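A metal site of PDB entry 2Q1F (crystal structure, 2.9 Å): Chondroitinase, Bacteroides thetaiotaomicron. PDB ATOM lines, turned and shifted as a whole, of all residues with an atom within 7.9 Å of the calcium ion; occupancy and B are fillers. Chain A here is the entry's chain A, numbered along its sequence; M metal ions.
Of the 22 residues printed, 5 come within 4 Å of the calcium ion.
The calcium ion is bound by O of Asp 50 (2.3 Å), O of Ser 24 (2.3 Å), OE1 of Glu 26 (2.4 Å), O of His 53 (2.4 Å), OD2 of Asp 161 (2.6 Å), OD1 of Asp 161 (2.7 Å) and OG of Ser 24 (2.8 Å). The calcium ion has seven donor atoms within binding distance. Slightly farther from the calcium ion lies the side-chain carboxylate (OD1) of Asp 50 (3.1 Å).
The backbone NH (N) of Lys 52 is in hydrogen-bond range of the side-chain carboxylate (OE2) of Glu 26 (2.9 Å). The side-chain carboxylate (OD1) of Asp 161 sits close to the backbone NH (N) of Lys 49, 2.8 Å away.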
ATOM      1  N   GLN A  15     -25.859  21.170 -36.717  1.00  0.00           N
ATOM      2  CA  GLN A  15     -27.145  21.413 -36.058  1.00  0.00           C
ATOM      3  C   GLN A  15     -28.161  21.948 -37.067  1.00  0.00           C
ATOM      4  O   GLN A  15     -27.848  22.838 -37.869  1.00  0.00           O
ATOM      5  CB  GLN A  15     -27.004  22.389 -34.871  1.00  0.00           C
ATOM      6  CG  GLN A  15     -26.555  23.809 -35.220  1.00  0.00           C
ATOM      7  CD  GLN A  15     -26.850  24.820 -34.116  1.00  0.00           C
ATOM      8  OE1 GLN A  15     -25.927  25.433 -33.564  1.00  0.00           O
ATOM      9  NE2 GLN A  15     -28.129  25.000 -33.781  1.00  0.00           N
ATOM     10  N   MET A  22     -32.099  29.998 -30.575  1.00  0.00           N
ATOM     11  CA  MET A  22     -31.802  28.569 -30.542  1.00  0.00           C
ATOM     12  C   MET A  22     -30.469  28.300 -29.853  1.00  0.00           C
ATOM     13  O   MET A  22     -29.410  28.769 -30.308  1.00  0.00           O
ATOM     14  CB  MET A  22     -31.824  28.010 -31.980  1.00  0.00           C
ATOM     15  CG  MET A  22     -31.150  26.651 -32.180  1.00  0.00           C
ATOM     16  SD  MET A  22     -32.337  25.114 -31.998  1.00  0.00           S
ATOM     17  CE  MET A  22     -32.343  24.964 -30.074  1.00  0.00           C
ATOM     18  N   PHE A  23     -30.518  27.557 -28.747  1.00  0.00           N
ATOM     19  CA  PHE A  23     -29.325  27.135 -28.020  1.00  0.00           C
ATOM     20  C   PHE A  23     -29.086  25.635 -28.189  1.00  0.00           C
ATOM     21  O   PHE A  23     -29.859  24.809 -27.719  1.00  0.00           O
ATOM     22  CB  PHE A  23     -29.471  27.467 -26.527  1.00  0.00           C
ATOM     23  CG  PHE A  23     -29.251  28.912 -26.198  1.00  0.00           C
ATOM     24  CD1 PHE A  23     -28.019  29.356 -25.758  1.00  0.00           C
ATOM     25  CD2 PHE A  23     -30.287  29.834 -26.329  1.00  0.00           C
ATOM     26  CE1 PHE A  23     -27.811  30.697 -25.454  1.00  0.00           C
ATOM     27  CE2 PHE A  23     -30.094  31.178 -26.039  1.00  0.00           C
ATOM     28  CZ  PHE A  23     -28.852  31.609 -25.598  1.00  0.00           C
ATOM     29  N   SER A  24     -27.987  25.299 -28.866  1.00  0.00           N
ATOM     30  CA  SER A  24     -27.652  23.912 -29.171  1.00  0.00           C
ATOM     31  C   SER A  24     -26.245  23.521 -28.697  1.00  0.00           C
ATOM     32  O   SER A  24     -25.871  22.343 -28.745  1.00  0.00           O
ATOM     33  CB  SER A  24     -27.807  23.668 -30.676  1.00  0.00           C
ATOM     34  OG  SER A  24     -27.339  22.392 -31.036  1.00  0.00           O
ATOM     35  N   PHE A  25     -25.488  24.510 -28.219  1.00  0.00           N
ATOM     36  CA  PHE A  25     -24.188  24.310 -27.554  1.00  0.00           C
ATOM     37  C   PHE A  25     -23.134  23.598 -28.409  1.00  0.00           C
ATOM     38  O   PHE A  25     -22.393  22.755 -27.918  1.00  0.00           O
ATOM     39  CB  PHE A  25     -24.375  23.574 -26.216  1.00  0.00           C
ATOM     40  CG  PHE A  25     -25.532  24.082 -25.394  1.00  0.00           C
ATOM     41  CD1 PHE A  25     -25.451  25.304 -24.743  1.00  0.00           C
ATOM     42  CD2 PHE A  25     -26.695  23.339 -25.275  1.00  0.00           C
ATOM     43  CE1 PHE A  25     -26.522  25.778 -23.987  1.00  0.00           C
ATOM     44  CE2 PHE A  25     -27.769  23.802 -24.532  1.00  0.00           C
ATOM     45  CZ  PHE A  25     -27.686  25.034 -23.882  1.00  0.00           C
ATOM     46  N   GLU A  26     -23.066  23.956 -29.693  1.00  0.00           N
ATOM     47  CA  GLU A  26     -22.141  23.276 -30.591  1.00  0.00           C
ATOM     48  C   GLU A  26     -20.782  23.974 -30.689  1.00  0.00           C
ATOM     49  O   GLU A  26     -19.912  23.549 -31.445  1.00  0.00           O
ATOM     50  CB  GLU A  26     -22.761  23.079 -31.983  1.00  0.00           C
ATOM     51  CG  GLU A  26     -23.961  22.141 -32.007  1.00  0.00           C
ATOM     52  CD  GLU A  26     -23.685  20.796 -31.342  1.00  0.00           C
ATOM     53  OE1 GLU A  26     -24.498  20.386 -30.487  1.00  0.00           O
ATOM     54  OE2 GLU A  26     -22.670  20.149 -31.675  1.00  0.00           O
ATOM     55  N   GLU A  27     -20.612  25.029 -29.899  1.00  0.00           N
ATOM     56  CA  GLU A  27     -19.371  25.787 -29.872  1.00  0.00           C
ATOM     57  C   GLU A  27     -18.447  25.282 -28.761  1.00  0.00           C
ATOM     58  O   GLU A  27     -18.925  24.793 -27.742  1.00  0.00           O
ATOM     59  CB  GLU A  27     -19.664  27.282 -29.703  1.00  0.00           C
ATOM     60  CG  GLU A  27     -20.528  27.907 -30.811  1.00  0.00           C
ATOM     61  CD  GLU A  27     -20.058  27.540 -32.229  1.00  0.00           C
ATOM     62  OE1 GLU A  27     -18.829  27.613 -32.507  1.00  0.00           O
ATOM     63  OE2 GLU A  27     -20.921  27.190 -33.061  1.00  0.00           O
ATOM     64  N   SER A  44     -20.648  18.826 -23.102  1.00  0.00           N
ATOM     65  CA  SER A  44     -20.480  17.378 -23.108  1.00  0.00           C
ATOM     66  C   SER A  44     -20.869  16.753 -24.436  1.00  0.00           C
ATOM     67  O   SER A  44     -21.832  17.192 -25.072  1.00  0.00           O
ATOM     68  CB  SER A  44     -21.309  16.755 -21.983  1.00  0.00           C
ATOM     69  OG  SER A  44     -21.404  15.346 -22.138  1.00  0.00           O
ATOM     70  N   HIS A  47     -24.103  13.026 -24.549  1.00  0.00           N
ATOM     71  CA  HIS A  47     -25.511  13.020 -24.925  1.00  0.00           C
ATOM     72  C   HIS A  47     -25.820  14.248 -25.770  1.00  0.00           C
ATOM     73  O   HIS A  47     -25.262  15.320 -25.524  1.00  0.00           O
ATOM     74  CB  HIS A  47     -26.407  13.008 -23.686  1.00  0.00           C
ATOM     75  CG  HIS A  47     -26.066  11.935 -22.702  1.00  0.00           C
ATOM     76  ND1 HIS A  47     -26.256  10.594 -22.965  1.00  0.00           N
ATOM     77  CD2 HIS A  47     -25.548  11.997 -21.457  1.00  0.00           C
ATOM     78  CE1 HIS A  47     -25.864   9.880 -21.924  1.00  0.00           C
ATOM     79  NE2 HIS A  47     -25.428  10.717 -20.985  1.00  0.00           N
ATOM     80  N   TYR A  48     -26.712  14.097 -26.758  1.00  0.00           N
ATOM     81  CA  TYR A  48     -27.074  15.196 -27.663  1.00  0.00           C
ATOM     82  C   TYR A  48     -28.381  14.916 -28.402  1.00  0.00           C
ATOM     83  O   TYR A  48     -28.626  13.798 -28.862  1.00  0.00           O
ATOM     84  CB  TYR A  48     -25.960  15.476 -28.674  1.00  0.00           C
ATOM     85  CG  TYR A  48     -25.524  14.270 -29.487  1.00  0.00           C
ATOM     86  CD1 TYR A  48     -24.560  13.403 -29.001  1.00  0.00           C
ATOM     87  CD2 TYR A  48     -26.086  14.021 -30.738  1.00  0.00           C
ATOM     88  CE1 TYR A  48     -24.155  12.288 -29.738  1.00  0.00           C
ATOM     89  CE2 TYR A  48     -25.680  12.915 -31.491  1.00  0.00           C
ATOM     90  CZ  TYR A  48     -24.718  12.061 -30.984  1.00  0.00           C
ATOM     91  OH  TYR A  48     -24.326  10.972 -31.715  1.00  0.00           O
ATOM     92  N   LYS A  49     -29.218  15.950 -28.510  1.00  0.00           N
ATOM     93  CA  LYS A  49     -30.487  15.838 -29.239  1.00  0.00           C
ATOM     94  C   LYS A  49     -30.407  16.528 -30.617  1.00  0.00           C
ATOM     95  O   LYS A  49     -31.202  16.224 -31.505  1.00  0.00           O
ATOM     96  CB  LYS A  49     -31.649  16.379 -28.420  1.00  0.00           C
ATOM     97  CG  LYS A  49     -33.020  16.025 -28.973  1.00  0.00           C
ATOM     98  CD  LYS A  49     -33.351  14.560 -28.792  1.00  0.00           C
ATOM     99  CE  LYS A  49     -34.624  14.205 -29.542  1.00  0.00           C
ATOM    100  NZ  LYS A  49     -35.152  12.876 -29.154  1.00  0.00           N
ATOM    101  N   ASP A  50     -29.461  17.447 -30.767  1.00  0.00           N
ATOM    102  CA  ASP A  50     -29.095  17.955 -32.073  1.00  0.00           C
ATOM    103  C   ASP A  50     -27.628  18.377 -32.097  1.00  0.00           C
ATOM    104  O   ASP A  50     -27.062  18.735 -31.062  1.00  0.00           O
ATOM    105  CB  ASP A  50     -30.029  19.101 -32.529  1.00  0.00           C
ATOM    106  CG  ASP A  50     -29.550  20.460 -32.105  1.00  0.00           C
ATOM    107  OD1 ASP A  50     -29.228  20.648 -30.910  1.00  0.00           O
ATOM    108  OD2 ASP A  50     -29.504  21.370 -32.961  1.00  0.00           O
ATOM    109  N   GLY A  51     -27.031  18.317 -33.277  1.00  0.00           N
ATOM    110  CA  GLY A  51     -25.591  18.515 -33.401  1.00  0.00           C
ATOM    111  C   GLY A  51     -24.894  17.308 -32.816  1.00  0.00           C
ATOM    112  O   GLY A  51     -25.256  16.162 -33.108  1.00  0.00           O
ATOM    113  N   LYS A  52     -23.912  17.552 -31.961  1.00  0.00           N
ATOM    114  CA  LYS A  52     -23.091  16.493 -31.412  1.00  0.00           C
ATOM    115  C   LYS A  52     -22.740  16.758 -29.948  1.00  0.00           C
ATOM    116  O   LYS A  52     -21.963  16.014 -29.334  1.00  0.00           O
ATOM    117  CB  LYS A  52     -21.817  16.325 -32.262  1.00  0.00           C
ATOM    118  CG  LYS A  52     -21.338  14.880 -32.437  1.00  0.00           C
ATOM    119  CD  LYS A  52     -22.378  13.981 -33.122  1.00  0.00           C
ATOM    120  CE  LYS A  52     -22.465  14.199 -34.632  1.00  0.00           C
ATOM    121  NZ  LYS A  52     -21.402  13.486 -35.388  1.00  0.00           N
ATOM    122  N   HIS A  53     -23.327  17.821 -29.383  1.00  0.00           N
ATOM    123  CA  HIS A  53     -23.022  18.265 -28.029  1.00  0.00           C
ATOM    124  C   HIS A  53     -24.264  18.700 -27.234  1.00  0.00           C
ATOM    125  O   HIS A  53     -25.318  18.986 -27.795  1.00  0.00           O
ATOM    126  CB  HIS A  53     -22.007  19.410 -28.049  1.00  0.00           C
ATOM    127  CG  HIS A  53     -20.725  19.063 -28.714  1.00  0.00           C
ATOM    128  ND1 HIS A  53     -19.729  18.350 -28.087  1.00  0.00           N
ATOM    129  CD2 HIS A  53     -20.255  19.337 -29.964  1.00  0.00           C
ATOM    130  CE1 HIS A  53     -18.700  18.196 -28.908  1.00  0.00           C
ATOM    131  NE2 HIS A  53     -19.000  18.785 -30.057  1.00  0.00           N
ATOM    132  N   SER A  54     -24.117  18.735 -25.911  1.00  0.00           N
ATOM    133  CA  SER A  54     -25.150  19.265 -25.029  1.00  0.00           C
ATOM    134  C   SER A  54     -24.520  19.962 -23.816  1.00  0.00           C
ATOM    135  O   SER A  54     -23.308  19.861 -23.592  1.00  0.00           O
ATOM    136  CB  SER A  54     -26.109  18.178 -24.570  1.00  0.00           C
ATOM    137  OG  SER A  54     -25.474  17.269 -23.680  1.00  0.00           O
ATOM    138  N   LEU A  55     -25.348  20.660 -23.047  1.00  0.00           N
ATOM    139  CA  LEU A  55     -24.906  21.358 -21.860  1.00  0.00           C
ATOM    140  C   LEU A  55     -25.033  20.488 -20.611  1.00  0.00           C
ATOM    141  O   LEU A  55     -26.145  20.167 -20.184  1.00  0.00           O
ATOM    142  CB  LEU A  55     -25.690  22.654 -21.669  1.00  0.00           C
ATOM    143  CG  LEU A  55     -25.371  23.489 -20.428  1.00  0.00           C
ATOM    144  CD1 LEU A  55     -23.891  23.833 -20.376  1.00  0.00           C
ATOM    145  CD2 LEU A  55     -26.230  24.737 -20.381  1.00  0.00           C
ATOM    146  N   TRP A 125     -33.631  10.920 -22.838  1.00  0.00           N
ATOM    147  CA  TRP A 125     -34.132  12.220 -23.306  1.00  0.00           C
ATOM    148  C   TRP A 125     -35.638  12.356 -23.103  1.00  0.00           C
ATOM    149  O   TRP A 125     -36.395  11.415 -23.362  1.00  0.00           O
ATOM    150  CB  TRP A 125     -33.814  12.416 -24.787  1.00  0.00           C
ATOM    151  CG  TRP A 125     -32.385  12.762 -25.100  1.00  0.00           C
ATOM    152  CD1 TRP A 125     -31.470  11.961 -25.730  1.00  0.00           C
ATOM    153  CD2 TRP A 125     -31.714  13.986 -24.797  1.00  0.00           C
ATOM    154  NE1 TRP A 125     -30.266  12.619 -25.840  1.00  0.00           N
ATOM    155  CE2 TRP A 125     -30.389  13.860 -25.271  1.00  0.00           C
ATOM    156  CE3 TRP A 125     -32.101  15.175 -24.175  1.00  0.00           C
ATOM    157  CZ2 TRP A 125     -29.447  14.888 -25.136  1.00  0.00           C
ATOM    158  CZ3 TRP A 125     -31.169  16.196 -24.045  1.00  0.00           C
ATOM    159  CH2 TRP A 125     -29.859  16.042 -24.522  1.00  0.00           C
ATOM    160  N   ILE A 160     -28.710  19.395 -20.962  1.00  0.00           N
ATOM    161  CA  ILE A 160     -29.677  20.248 -21.654  1.00  0.00           C
ATOM    162  C   ILE A 160     -29.269  20.462 -23.112  1.00  0.00           C
ATOM    163  O   ILE A 160     -28.112  20.808 -23.398  1.00  0.00           O
ATOM    164  CB  ILE A 160     -29.808  21.626 -20.931  1.00  0.00           C
ATOM    165  CG1 ILE A 160     -30.290  21.421 -19.492  1.00  0.00           C
ATOM    166  CG2 ILE A 160     -30.759  22.551 -21.688  1.00  0.00           C
ATOM    167  CD1 ILE A 160     -30.131  22.619 -18.591  1.00  0.00           C
ATOM    168  N   ASP A 161     -30.208  20.251 -24.026  1.00  0.00           N
ATOM    169  CA  ASP A 161     -29.979  20.502 -25.450  1.00  0.00           C
ATOM    170  C   ASP A 161     -31.281  20.919 -26.141  1.00  0.00           C
ATOM    171  O   ASP A 161     -32.371  20.723 -25.583  1.00  0.00           O
ATOM    172  CB  ASP A 161     -29.413  19.263 -26.126  1.00  0.00           C
ATOM    173  CG  ASP A 161     -28.719  19.580 -27.430  1.00  0.00           C
ATOM    174  OD1 ASP A 161     -28.452  18.637 -28.214  1.00  0.00           O
ATOM    175  OD2 ASP A 161     -28.438  20.766 -27.695  1.00  0.00           O
ATOM    176  N   HIS A 162     -31.152  21.491 -27.336  1.00  0.00           N
ATOM    177  CA  HIS A 162     -32.299  21.899 -28.153  1.00  0.00           C
ATOM    178  C   HIS A 162     -33.192  22.868 -27.384  1.00  0.00           C
ATOM    179  O   HIS A 162     -34.380  22.616 -27.181  1.00  0.00           O
ATOM    180  CB  HIS A 162     -33.079  20.673 -28.643  1.00  0.00           C
ATOM    181  CG  HIS A 162     -34.031  20.945 -29.760  1.00  0.00           C
ATOM    182  ND1 HIS A 162     -33.766  20.601 -31.067  1.00  0.00           N
ATOM    183  CD2 HIS A 162     -35.269  21.490 -29.769  1.00  0.00           C
ATOM    184  CE1 HIS A 162     -34.786  20.946 -31.831  1.00  0.00           C
ATOM    185  NE2 HIS A 162     -35.709  21.483 -31.064  1.00  0.00           N
ATOM    186  N   LEU A 163     -32.602  23.977 -26.931  1.00  0.00           N
ATOM    187  CA  LEU A 163     -33.346  24.974 -26.176  1.00  0.00           C
ATOM    188  C   LEU A 163     -33.740  26.158 -27.069  1.00  0.00           C
ATOM    189  O   LEU A 163     -32.880  26.906 -27.537  1.00  0.00           O
ATOM    190  CB  LEU A 163     -32.539  25.451 -24.960  1.00  0.00           C
ATOM    191  CG  LEU A 163     -33.191  26.353 -23.894  1.00  0.00           C
ATOM    192  CD1 LEU A 163     -32.515  26.171 -22.549  1.00  0.00           C
ATOM    193  CD2 LEU A 163     -33.205  27.832 -24.289  1.00  0.00           C
HETATM  194 CA    CA M   1     -26.594  20.220 -29.388  1.00  0.00          CA
